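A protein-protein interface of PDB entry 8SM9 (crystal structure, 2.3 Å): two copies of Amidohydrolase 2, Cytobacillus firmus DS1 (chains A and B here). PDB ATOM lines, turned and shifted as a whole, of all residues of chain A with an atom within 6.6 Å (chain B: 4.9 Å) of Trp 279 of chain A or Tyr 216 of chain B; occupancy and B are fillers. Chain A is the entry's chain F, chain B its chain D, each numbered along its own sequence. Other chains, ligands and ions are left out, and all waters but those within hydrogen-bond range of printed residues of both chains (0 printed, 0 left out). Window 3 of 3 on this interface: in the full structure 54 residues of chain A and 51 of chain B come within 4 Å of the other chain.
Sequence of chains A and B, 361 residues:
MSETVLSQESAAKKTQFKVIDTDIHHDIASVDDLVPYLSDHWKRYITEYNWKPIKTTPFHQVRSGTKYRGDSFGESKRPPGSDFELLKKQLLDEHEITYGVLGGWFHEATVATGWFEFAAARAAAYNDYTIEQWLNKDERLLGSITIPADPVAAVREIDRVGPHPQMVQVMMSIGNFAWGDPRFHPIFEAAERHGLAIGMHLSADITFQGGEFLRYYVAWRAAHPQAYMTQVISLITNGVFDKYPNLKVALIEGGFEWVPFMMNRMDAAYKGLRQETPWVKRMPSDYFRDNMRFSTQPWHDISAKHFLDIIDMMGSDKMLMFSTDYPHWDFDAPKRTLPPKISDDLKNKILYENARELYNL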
ATOM      1  N   PRO A 182      -6.415 -27.121 -33.510  1.00  0.00           N
ATOM      2  CA  PRO A 182      -5.580 -28.267 -33.889  1.00  0.00           C
ATOM      3  C   PRO A 182      -6.168 -29.105 -34.997  1.00  0.00           C
ATOM      4  O   PRO A 182      -5.418 -29.738 -35.757  1.00  0.00           O
ATOM      5  CB  PRO A 182      -5.476 -29.065 -32.579  1.00  0.00           C
ATOM      6  CG  PRO A 182      -6.331 -28.337 -31.563  1.00  0.00           C
ATOM      7  CD  PRO A 182      -6.450 -26.942 -32.052  1.00  0.00           C
ATOM      8  N   ILE A 236      -2.138 -17.927 -32.389  1.00  0.00           N
ATOM      9  CA  ILE A 236      -1.080 -17.824 -31.394  1.00  0.00           C
ATOM     10  C   ILE A 236      -1.271 -18.875 -30.310  1.00  0.00           C
ATOM     11  O   ILE A 236      -0.361 -19.669 -30.046  1.00  0.00           O
ATOM     12  CB  ILE A 236      -1.031 -16.403 -30.807  1.00  0.00           C
ATOM     13  CG1 ILE A 236      -0.353 -15.447 -31.809  1.00  0.00           C
ATOM     14  CG2 ILE A 236      -0.289 -16.425 -29.507  1.00  0.00           C
ATOM     15  CD1 ILE A 236      -0.602 -13.969 -31.561  1.00  0.00           C
ATOM     16  N   THR A 237      -2.482 -18.931 -29.708  1.00  0.00           N
ATOM     17  CA  THR A 237      -2.747 -19.737 -28.519  1.00  0.00           C
ATOM     18  C   THR A 237      -2.801 -21.226 -28.795  1.00  0.00           C
ATOM     19  O   THR A 237      -2.603 -22.024 -27.875  1.00  0.00           O
ATOM     20  CB  THR A 237      -4.067 -19.317 -27.857  1.00  0.00           C
ATOM     21  OG1 THR A 237      -5.121 -19.306 -28.829  1.00  0.00           O
ATOM     22  CG2 THR A 237      -3.941 -17.928 -27.256  1.00  0.00           C
ATOM     23  N   ASN A 238      -3.097 -21.626 -30.010  1.00  0.00           N
ATOM     24  CA  ASN A 238      -2.941 -23.025 -30.334  1.00  0.00           C
ATOM     25  C   ASN A 238      -1.517 -23.353 -30.747  1.00  0.00           C
ATOM     26  O   ASN A 238      -1.250 -24.484 -31.162  1.00  0.00           O
ATOM     27  CB  ASN A 238      -3.926 -23.407 -31.443  1.00  0.00           C
ATOM     28  CG  ASN A 238      -5.364 -23.543 -30.940  1.00  0.00           C
ATOM     29  OD1 ASN A 238      -5.675 -24.401 -30.104  1.00  0.00           O
ATOM     30  ND2 ASN A 238      -6.246 -22.689 -31.453  1.00  0.00           N
ATOM     31  N   GLY A 239      -0.608 -22.388 -30.681  1.00  0.00           N
ATOM     32  CA  GLY A 239       0.781 -22.638 -31.038  1.00  0.00           C
ATOM     33  C   GLY A 239       1.039 -22.988 -32.486  1.00  0.00           C
ATOM     34  O   GLY A 239       1.867 -23.859 -32.768  1.00  0.00           O
ATOM     35  N   VAL A 240       0.376 -22.313 -33.420  1.00  0.00           N
ATOM     36  CA  VAL A 240       0.599 -22.621 -34.826  1.00  0.00           C
ATOM     37  C   VAL A 240       1.998 -22.195 -35.246  1.00  0.00           C
ATOM     38  O   VAL A 240       2.663 -22.871 -36.042  1.00  0.00           O
ATOM     39  CB  VAL A 240      -0.487 -21.954 -35.686  1.00  0.00           C
ATOM     40  CG1 VAL A 240      -0.199 -22.117 -37.178  1.00  0.00           C
ATOM     41  CG2 VAL A 240      -1.818 -22.542 -35.321  1.00  0.00           C
ATOM     42  N   ASP A 242       4.684 -21.635 -33.095  1.00  0.00           N
ATOM     43  CA  ASP A 242       5.681 -22.484 -32.448  1.00  0.00           C
ATOM     44  C   ASP A 242       5.852 -23.812 -33.185  1.00  0.00           C
ATOM     45  O   ASP A 242       6.960 -24.359 -33.214  1.00  0.00           O
ATOM     46  CB  ASP A 242       5.310 -22.741 -30.990  1.00  0.00           C
ATOM     47  CG  ASP A 242       4.974 -21.466 -30.234  1.00  0.00           C
ATOM     48  OD1 ASP A 242       5.902 -20.832 -29.683  1.00  0.00           O
ATOM     49  OD2 ASP A 242       3.775 -21.100 -30.173  1.00  0.00           O
ATOM     50  N   LYS A 243       4.784 -24.343 -33.789  1.00  0.00           N
ATOM     51  CA  LYS A 243       4.907 -25.565 -34.581  1.00  0.00           C
ATOM     52  C   LYS A 243       5.575 -25.302 -35.924  1.00  0.00           C
ATOM     53  O   LYS A 243       6.355 -26.132 -36.402  1.00  0.00           O
ATOM     54  CB  LYS A 243       3.533 -26.192 -34.801  1.00  0.00           C
ATOM     55  CG  LYS A 243       3.276 -27.440 -33.989  1.00  0.00           C
ATOM     56  CD  LYS A 243       1.986 -28.125 -34.425  1.00  0.00           C
ATOM     57  CE  LYS A 243       1.069 -28.325 -33.232  1.00  0.00           C
ATOM     58  NZ  LYS A 243       0.045 -29.334 -33.508  1.00  0.00           N
ATOM     59  N   TYR A 270      -0.576 -12.901 -21.219  1.00  0.00           N
ATOM     60  CA  TYR A 270       0.311 -14.053 -21.233  1.00  0.00           C
ATOM     61  C   TYR A 270       1.341 -14.020 -20.115  1.00  0.00           C
ATOM     62  O   TYR A 270       1.731 -15.088 -19.621  1.00  0.00           O
ATOM     63  CB  TYR A 270       0.994 -14.171 -22.586  1.00  0.00           C
ATOM     64  CG  TYR A 270       0.409 -15.310 -23.354  1.00  0.00           C
ATOM     65  CD1 TYR A 270      -0.726 -15.136 -24.137  1.00  0.00           C
ATOM     66  CD2 TYR A 270       0.957 -16.572 -23.254  1.00  0.00           C
ATOM     67  CE1 TYR A 270      -1.266 -16.175 -24.826  1.00  0.00           C
ATOM     68  CE2 TYR A 270       0.431 -17.610 -23.930  1.00  0.00           C
ATOM     69  CZ  TYR A 270      -0.681 -17.415 -24.716  1.00  0.00           C
ATOM     70  OH  TYR A 270      -1.191 -18.495 -25.390  1.00  0.00           O
ATOM     71  N   ARG A 274       0.389 -18.026 -18.850  1.00  0.00           N
ATOM     72  CA  ARG A 274       0.977 -18.754 -19.977  1.00  0.00           C
ATOM     73  C   ARG A 274       1.003 -20.264 -19.758  1.00  0.00           C
ATOM     74  O   ARG A 274       1.027 -21.019 -20.738  1.00  0.00           O
ATOM     75  CB  ARG A 274       2.392 -18.235 -20.256  1.00  0.00           C
ATOM     76  CG  ARG A 274       3.167 -19.038 -21.298  1.00  0.00           C
ATOM     77  CD  ARG A 274       4.614 -18.712 -21.181  1.00  0.00           C
ATOM     78  NE  ARG A 274       4.813 -17.318 -21.533  1.00  0.00           N
ATOM     79  CZ  ARG A 274       5.041 -16.889 -22.767  1.00  0.00           C
ATOM     80  NH1 ARG A 274       5.165 -17.730 -23.784  1.00  0.00           N
ATOM     81  NH2 ARG A 274       5.153 -15.583 -22.988  1.00  0.00           N
ATOM     82  N   GLN A 275       0.991 -20.728 -18.497  1.00  0.00           N
ATOM     83  CA  GLN A 275       1.005 -22.170 -18.224  1.00  0.00           C
ATOM     84  C   GLN A 275      -0.256 -22.877 -18.723  1.00  0.00           C
ATOM     85  O   GLN A 275      -0.281 -24.114 -18.805  1.00  0.00           O
ATOM     86  CB  GLN A 275       1.186 -22.442 -16.721  1.00  0.00           C
ATOM     87  CG  GLN A 275       1.936 -21.363 -15.950  1.00  0.00           C
ATOM     88  CD  GLN A 275       1.025 -20.408 -15.179  1.00  0.00           C
ATOM     89  OE1 GLN A 275      -0.113 -20.140 -15.584  1.00  0.00           O
ATOM     90  NE2 GLN A 275       1.535 -19.883 -14.059  1.00  0.00           N
ATOM     91  N   GLU A 276      -1.310 -22.125 -19.041  1.00  0.00           N
ATOM     92  CA  GLU A 276      -2.484 -22.745 -19.640  1.00  0.00           C
ATOM     93  C   GLU A 276      -2.178 -23.246 -21.047  1.00  0.00           C
ATOM     94  O   GLU A 276      -2.668 -24.306 -21.458  1.00  0.00           O
ATOM     95  CB  GLU A 276      -3.647 -21.758 -19.647  1.00  0.00           C
ATOM     96  CG  GLU A 276      -4.854 -22.226 -20.398  1.00  0.00           C
ATOM     97  CD  GLU A 276      -5.951 -21.212 -20.289  1.00  0.00           C
ATOM     98  OE1 GLU A 276      -5.583 -20.013 -20.185  1.00  0.00           O
ATOM     99  OE2 GLU A 276      -7.149 -21.604 -20.281  1.00  0.00           O
ATOM    100  N   THR A 277      -1.359 -22.503 -21.795  1.00  0.00           N
ATOM    101  CA  THR A 277      -0.926 -22.881 -23.140  1.00  0.00           C
ATOM    102  C   THR A 277       0.604 -22.966 -23.173  1.00  0.00           C
ATOM    103  O   THR A 277       1.279 -22.113 -23.770  1.00  0.00           O
ATOM    104  CB  THR A 277      -1.450 -21.893 -24.186  1.00  0.00           C
ATOM    105  OG1 THR A 277      -0.927 -20.579 -23.924  1.00  0.00           O
ATOM    106  CG2 THR A 277      -2.978 -21.842 -24.169  1.00  0.00           C
ATOM    107  N   PRO A 278       1.181 -24.004 -22.557  1.00  0.00           N
ATOM    108  CA  PRO A 278       2.646 -24.056 -22.415  1.00  0.00           C
ATOM    109  C   PRO A 278       3.402 -24.251 -23.727  1.00  0.00           C
ATOM    110  O   PRO A 278       4.635 -24.126 -23.719  1.00  0.00           O
ATOM    111  CB  PRO A 278       2.859 -25.245 -21.466  1.00  0.00           C
ATOM    112  CG  PRO A 278       1.634 -26.112 -21.644  1.00  0.00           C
ATOM    113  CD  PRO A 278       0.513 -25.157 -21.915  1.00  0.00           C
ATOM    114  N   TRP A 279       2.723 -24.539 -24.844  1.00  0.00           N
ATOM    115  CA  TRP A 279       3.413 -24.671 -26.124  1.00  0.00           C
ATOM    116  C   TRP A 279       3.796 -23.319 -26.711  1.00  0.00           C
ATOM    117  O   TRP A 279       4.716 -23.255 -27.536  1.00  0.00           O
ATOM    118  CB  TRP A 279       2.551 -25.444 -27.135  1.00  0.00           C
ATOM    119  CG  TRP A 279       1.114 -25.040 -27.065  1.00  0.00           C
ATOM    120  CD1 TRP A 279       0.512 -24.038 -27.771  1.00  0.00           C
ATOM    121  CD2 TRP A 279       0.100 -25.598 -26.214  1.00  0.00           C
ATOM    122  NE1 TRP A 279      -0.809 -23.938 -27.414  1.00  0.00           N
ATOM    123  CE2 TRP A 279      -1.086 -24.881 -26.457  1.00  0.00           C
ATOM    124  CE3 TRP A 279       0.088 -26.617 -25.257  1.00  0.00           C
ATOM    125  CZ2 TRP A 279      -2.279 -25.156 -25.787  1.00  0.00           C
ATOM    126  CZ3 TRP A 279      -1.101 -26.893 -24.596  1.00  0.00           C
ATOM    127  CH2 TRP A 279      -2.265 -26.166 -24.865  1.00  0.00           C
ATOM    128  N   VAL A 280       3.116 -22.247 -26.311  1.00  0.00           N
ATOM    129  CA  VAL A 280       3.455 -20.908 -26.784  1.00  0.00           C
ATOM    130  C   VAL A 280       4.752 -20.492 -26.095  1.00  0.00           C
ATOM    131  O   VAL A 280       4.766 -20.178 -24.900  1.00  0.00           O
ATOM    132  CB  VAL A 280       2.321 -19.911 -26.511  1.00  0.00           C
ATOM    133  CG1 VAL A 280       2.643 -18.535 -27.064  1.00  0.00           C
ATOM    134  CG2 VAL A 280       1.065 -20.401 -27.124  1.00  0.00           C
ATOM    135  N   LYS A 281       5.850 -20.491 -26.854  1.00  0.00           N
ATOM    136  CA  LYS A 281       7.167 -20.243 -26.292  1.00  0.00           C
ATOM    137  C   LYS A 281       7.581 -18.780 -26.345  1.00  0.00           C
ATOM    138  O   LYS A 281       8.452 -18.370 -25.566  1.00  0.00           O
ATOM    139  CB  LYS A 281       8.200 -21.099 -27.026  1.00  0.00           C
ATOM    140  CG  LYS A 281       8.076 -22.593 -26.719  1.00  0.00           C
ATOM    141  CD  LYS A 281       7.579 -22.810 -25.295  1.00  0.00           C
ATOM    142  CE  LYS A 281       7.819 -24.229 -24.811  1.00  0.00           C
ATOM    143  NZ  LYS A 281       7.765 -25.211 -25.930  1.00  0.00           N
ATOM    144  N   ARG A 282       6.991 -17.984 -27.230  1.00  0.00           N
ATOM    145  CA  ARG A 282       7.400 -16.600 -27.405  1.00  0.00           C
ATOM    146  C   ARG A 282       6.371 -15.671 -26.782  1.00  0.00           C
ATOM    147  O   ARG A 282       5.423 -16.121 -26.135  1.00  0.00           O
ATOM    148  CB  ARG A 282       7.625 -16.296 -28.881  1.00  0.00           C
ATOM    149  CG  ARG A 282       8.473 -17.342 -29.562  1.00  0.00           C
ATOM    150  CD  ARG A 282       9.082 -16.821 -30.841  1.00  0.00           C
ATOM    151  NE  ARG A 282       9.788 -15.554 -30.674  1.00  0.00           N
ATOM    152  CZ  ARG A 282      10.081 -14.731 -31.675  1.00  0.00           C
ATOM    153  NH1 ARG A 282       9.691 -14.976 -32.918  1.00  0.00           N
ATOM    154  NH2 ARG A 282      10.780 -13.635 -31.427  1.00  0.00           N
ATOM    155  N   TYR A 287       5.055 -12.952 -32.342  1.00  0.00           N
ATOM    156  CA  TYR A 287       4.409 -13.596 -33.475  1.00  0.00           C
ATOM    157  C   TYR A 287       3.814 -12.569 -34.418  1.00  0.00           C
ATOM    158  O   TYR A 287       3.849 -12.750 -35.641  1.00  0.00           O
ATOM    159  CB  TYR A 287       3.318 -14.537 -32.988  1.00  0.00           C
ATOM    160  CG  TYR A 287       3.785 -15.584 -32.022  1.00  0.00           C
ATOM    161  CD1 TYR A 287       4.599 -16.621 -32.443  1.00  0.00           C
ATOM    162  CD2 TYR A 287       3.406 -15.547 -30.685  1.00  0.00           C
ATOM    163  CE1 TYR A 287       5.027 -17.604 -31.562  1.00  0.00           C
ATOM    164  CE2 TYR A 287       3.823 -16.529 -29.798  1.00  0.00           C
ATOM    165  CZ  TYR A 287       4.630 -17.555 -30.248  1.00  0.00           C
ATOM    166  OH  TYR A 287       5.047 -18.540 -29.387  1.00  0.00           O
ATOM    167  N   PHE B  59     -13.905 -22.660 -18.805  1.00  0.00           N
ATOM    168  CA  PHE B  59     -12.522 -22.487 -18.309  1.00  0.00           C
ATOM    169  C   PHE B  59     -12.426 -21.291 -17.362  1.00  0.00           C
ATOM    170  O   PHE B  59     -13.430 -20.597 -17.180  1.00  0.00           O
ATOM    171  CB  PHE B  59     -11.558 -22.336 -19.488  1.00  0.00           C
ATOM    172  CG  PHE B  59     -12.079 -21.587 -20.684  1.00  0.00           C
ATOM    173  CD1 PHE B  59     -12.596 -20.311 -20.555  1.00  0.00           C
ATOM    174  CD2 PHE B  59     -12.024 -22.153 -21.944  1.00  0.00           C
ATOM    175  CE1 PHE B  59     -13.067 -19.624 -21.661  1.00  0.00           C
ATOM    176  CE2 PHE B  59     -12.494 -21.466 -23.050  1.00  0.00           C
ATOM    177  CZ  PHE B  59     -13.016 -20.204 -22.905  1.00  0.00           C
ATOM    178  N   PHE B 213     -15.973 -21.038 -27.699  1.00  0.00           N
ATOM    179  CA  PHE B 213     -15.326 -20.386 -26.570  1.00  0.00           C
ATOM    180  C   PHE B 213     -13.839 -20.133 -26.778  1.00  0.00           C
ATOM    181  O   PHE B 213     -13.216 -19.490 -25.923  1.00  0.00           O
ATOM    182  CB  PHE B 213     -15.518 -21.229 -25.305  1.00  0.00           C
ATOM    183  CG  PHE B 213     -16.791 -20.940 -24.579  1.00  0.00           C
ATOM    184  CD1 PHE B 213     -16.911 -19.795 -23.806  1.00  0.00           C
ATOM    185  CD2 PHE B 213     -17.864 -21.804 -24.668  1.00  0.00           C
ATOM    186  CE1 PHE B 213     -18.090 -19.511 -23.141  1.00  0.00           C
ATOM    187  CE2 PHE B 213     -19.051 -21.524 -24.006  1.00  0.00           C
ATOM    188  CZ  PHE B 213     -19.162 -20.379 -23.236  1.00  0.00           C
ATOM    189  N   LEU B 214     -13.256 -20.645 -27.863  1.00  0.00           N
ATOM    190  CA  LEU B 214     -11.840 -20.501 -28.197  1.00  0.00           C
ATOM    191  C   LEU B 214     -10.908 -21.302 -27.290  1.00  0.00           C
ATOM    192  O   LEU B 214      -9.746 -20.940 -27.157  1.00  0.00           O
ATOM    193  CB  LEU B 214     -11.413 -19.025 -28.218  1.00  0.00           C
ATOM    194  CG  LEU B 214     -12.225 -18.171 -29.197  1.00  0.00           C
ATOM    195  CD1 LEU B 214     -11.711 -16.755 -29.326  1.00  0.00           C
ATOM    196  CD2 LEU B 214     -12.246 -18.842 -30.568  1.00  0.00           C
ATOM    197  N   ARG B 215     -11.390 -22.377 -26.661  1.00  0.00           N
ATOM    198  CA  ARG B 215     -10.557 -23.454 -26.117  1.00  0.00           C
ATOM    199  C   ARG B 215      -9.795 -23.146 -24.822  1.00  0.00           C
ATOM    200  O   ARG B 215      -9.636 -24.033 -23.975  1.00  0.00           O
ATOM    201  CB  ARG B 215      -9.549 -23.908 -27.169  1.00  0.00           C
ATOM    202  CG  ARG B 215     -10.164 -24.322 -28.481  1.00  0.00           C
ATOM    203  CD  ARG B 215      -9.105 -24.932 -29.389  1.00  0.00           C
ATOM    204  NE  ARG B 215      -8.307 -25.876 -28.622  1.00  0.00           N
ATOM    205  CZ  ARG B 215      -8.373 -27.193 -28.752  1.00  0.00           C
ATOM    206  NH1 ARG B 215      -9.178 -27.759 -29.633  1.00  0.00           N
ATOM    207  NH2 ARG B 215      -7.601 -27.958 -27.987  1.00  0.00           N
ATOM    208  N   TYR B 216      -9.289 -21.924 -24.663  1.00  0.00           N
ATOM    209  CA  TYR B 216      -8.478 -21.539 -23.513  1.00  0.00           C
ATOM    210  C   TYR B 216      -8.988 -20.229 -22.926  1.00  0.00           C
ATOM    211  O   TYR B 216      -9.513 -19.373 -23.647  1.00  0.00           O
ATOM    212  CB  TYR B 216      -6.986 -21.424 -23.915  1.00  0.00           C
ATOM    213  CG  TYR B 216      -6.509 -22.656 -24.674  1.00  0.00           C
ATOM    214  CD1 TYR B 216      -6.357 -23.876 -24.024  1.00  0.00           C
ATOM    215  CD2 TYR B 216      -6.254 -22.607 -26.027  1.00  0.00           C
ATOM    216  CE1 TYR B 216      -5.953 -24.999 -24.695  1.00  0.00           C
ATOM    217  CE2 TYR B 216      -5.853 -23.736 -26.721  1.00  0.00           C
ATOM    218  CZ  TYR B 216      -5.703 -24.934 -26.048  1.00  0.00           C
ATOM    219  OH  TYR B 216      -5.294 -26.075 -26.715  1.00  0.00           O
ATOM    220  N   TYR B 217      -8.870 -20.086 -21.602  1.00  0.00           N
ATOM    221  CA  TYR B 217      -9.275 -18.825 -20.995  1.00  0.00           C
ATOM    222  C   TYR B 217      -8.420 -17.685 -21.517  1.00  0.00           C
ATOM    223  O   TYR B 217      -8.915 -16.573 -21.745  1.00  0.00           O
ATOM    224  CB  TYR B 217      -9.195 -18.870 -19.469  1.00  0.00           C
ATOM    225  CG  TYR B 217      -9.401 -17.487 -18.860  1.00  0.00           C
ATOM    226  CD1 TYR B 217     -10.673 -16.963 -18.695  1.00  0.00           C
ATOM    227  CD2 TYR B 217      -8.309 -16.689 -18.475  1.00  0.00           C
ATOM    228  CE1 TYR B 217     -10.870 -15.685 -18.149  1.00  0.00           C
ATOM    229  CE2 TYR B 217      -8.491 -15.408 -17.929  1.00  0.00           C
ATOM    230  CZ  TYR B 217      -9.782 -14.911 -17.764  1.00  0.00           C
ATOM    231  OH  TYR B 217      -9.985 -13.642 -17.223  1.00  0.00           O
ATOM    232  N   VAL B 218      -7.136 -17.947 -21.743  1.00  0.00           N
ATOM    233  CA  VAL B 218      -6.278 -16.854 -22.152  1.00  0.00           C
ATOM    234  C   VAL B 218      -6.699 -16.327 -23.522  1.00  0.00           C
ATOM    235  O   VAL B 218      -6.570 -15.127 -23.792  1.00  0.00           O
ATOM    236  CB  VAL B 218      -4.807 -17.297 -22.082  1.00  0.00           C
ATOM    237  CG1 VAL B 218      -4.508 -18.352 -23.115  1.00  0.00           C
ATOM    238  CG2 VAL B 218      -3.890 -16.089 -22.189  1.00  0.00           C
ATOM    239  N   ALA B 219      -7.271 -17.189 -24.376  1.00  0.00           N
ATOM    240  CA  ALA B 219      -7.785 -16.770 -25.679  1.00  0.00           C
ATOM    241  C   ALA B 219      -9.135 -16.079 -25.547  1.00  0.00           C
ATOM    242  O   ALA B 219      -9.359 -15.025 -26.159  1.00  0.00           O
ATOM    243  CB  ALA B 219      -7.902 -17.969 -26.625  1.00  0.00           C
ATOM    244  N   TRP B 220     -10.048 -16.671 -24.765  1.00  0.00           N
ATOM    245  CA  TRP B 220     -11.332 -16.040 -24.469  1.00  0.00           C
ATOM    246  C   TRP B 220     -11.144 -14.633 -23.913  1.00  0.00           C
ATOM    247  O   TRP B 220     -11.815 -13.685 -24.340  1.00  0.00           O
ATOM    248  CB  TRP B 220     -12.115 -16.918 -23.484  1.00  0.00           C
ATOM    249  CG  TRP B 220     -13.514 -16.427 -23.137  1.00  0.00           C
ATOM    250  CD1 TRP B 220     -14.700 -16.784 -23.752  1.00  0.00           C
ATOM    251  CD2 TRP B 220     -13.866 -15.518 -22.088  1.00  0.00           C
ATOM    252  NE1 TRP B 220     -15.760 -16.135 -23.148  1.00  0.00           N
ATOM    253  CE2 TRP B 220     -15.276 -15.359 -22.124  1.00  0.00           C
ATOM    254  CE3 TRP B 220     -13.128 -14.813 -21.125  1.00  0.00           C
ATOM    255  CZ2 TRP B 220     -15.954 -14.524 -21.234  1.00  0.00           C
ATOM    256  CZ3 TRP B 220     -13.803 -13.980 -20.245  1.00  0.00           C
ATOM    257  CH2 TRP B 220     -15.202 -13.843 -20.304  1.00  0.00           C
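No position is printed for both chains.
Of the 12 pairs that touch across the chains among the printed residues, none has its exchanged pair printed and touching as well.
Of the printed residues of chain B, Asn 238 of chain A touches Arg 215 (3.4 Å) and Tyr 216 (3.5 Å).
Gly 239 of chain A touches none of the printed residues of chain B.
Trp 279 of chain A touches one residue of chain B.
Tyr 216 of chain B touches just these residues of chain A: Thr 237, Asn 238, Glu 276, Thr 277 and Trp 279.
Printed residues of chain A within 4 Å of Ala 219 of chain B: Thr 237.
The nearest printed residue of chain B that does not touch Trp 279 of chain A is Arg 215 of chain B (6.4 Å).
The nearest residue of chain A that does not touch Tyr 216 of chain B is Pro 182 of chain A (5.4 Å).
Among the printed residues, pairs that only touch across the chains: Pro 182 of chain A with Arg 215 of chain B, Thr 237 of chain A with Tyr 216 of chain B, Thr 237 of chain A with Ala 219 of chain B, Asn 238 of chain A with Tyr 216 of chain B, Tyr 270 of chain A with Val 218 of chain B, Glu 276 of chain A with Tyr 216 of chain B, Thr 277 of chain A with Tyr 216 of chain B, Thr 277 of chain A with Val 218 of chain B and Trp 279 of chain A with Tyr 216 of chain B.
OG1 of Thr 277 of chain A is in hydrogen-bond range of OH of Tyr 270 of chain A (2.6 Å).
The side-chain hydroxyl (OH) of Tyr 216 of chain B lies within hydrogen-bond range of the guanidinium group (NH2) of Arg 215 of chain B.
The indole nitrogen (NE1) of Trp 279 of chain A sits at hydrogen-bond distance from the backbone carbonyl oxygen (O) of Thr 237 of chain A (2.7 Å).
The side-chain carboxylate of Glu 276 of chain A sits at hydrogen-bond distance from the backbone NH of Tyr 217 of chain B, 2.6 Å away.
The guanidinium group of Arg 215 of chain B is in hydrogen-bond range of the side-chain amide oxygen of Asn 238 of chain A (3.4 Å).
OE1 of Glu 276 of chain A lies within hydrogen-bond range of N of Val 218 of chain B (3.0 Å).
Of the 9 printed residues of chain B, 5 touch a printed residue of chain A.
Printed residues of chain B that touch a printed residue of chain A: Arg 215, Tyr 216, Tyr 217, Val 218 and Ala 219.
Hydrophobic or aromatic side chains of chain B within 4 Å of the printed part of chain A: Tyr 216, Tyr 217, Val 218 and Ala 219.
Of the 19 printed residues of chain A, 7 touch a printed residue of chain B.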
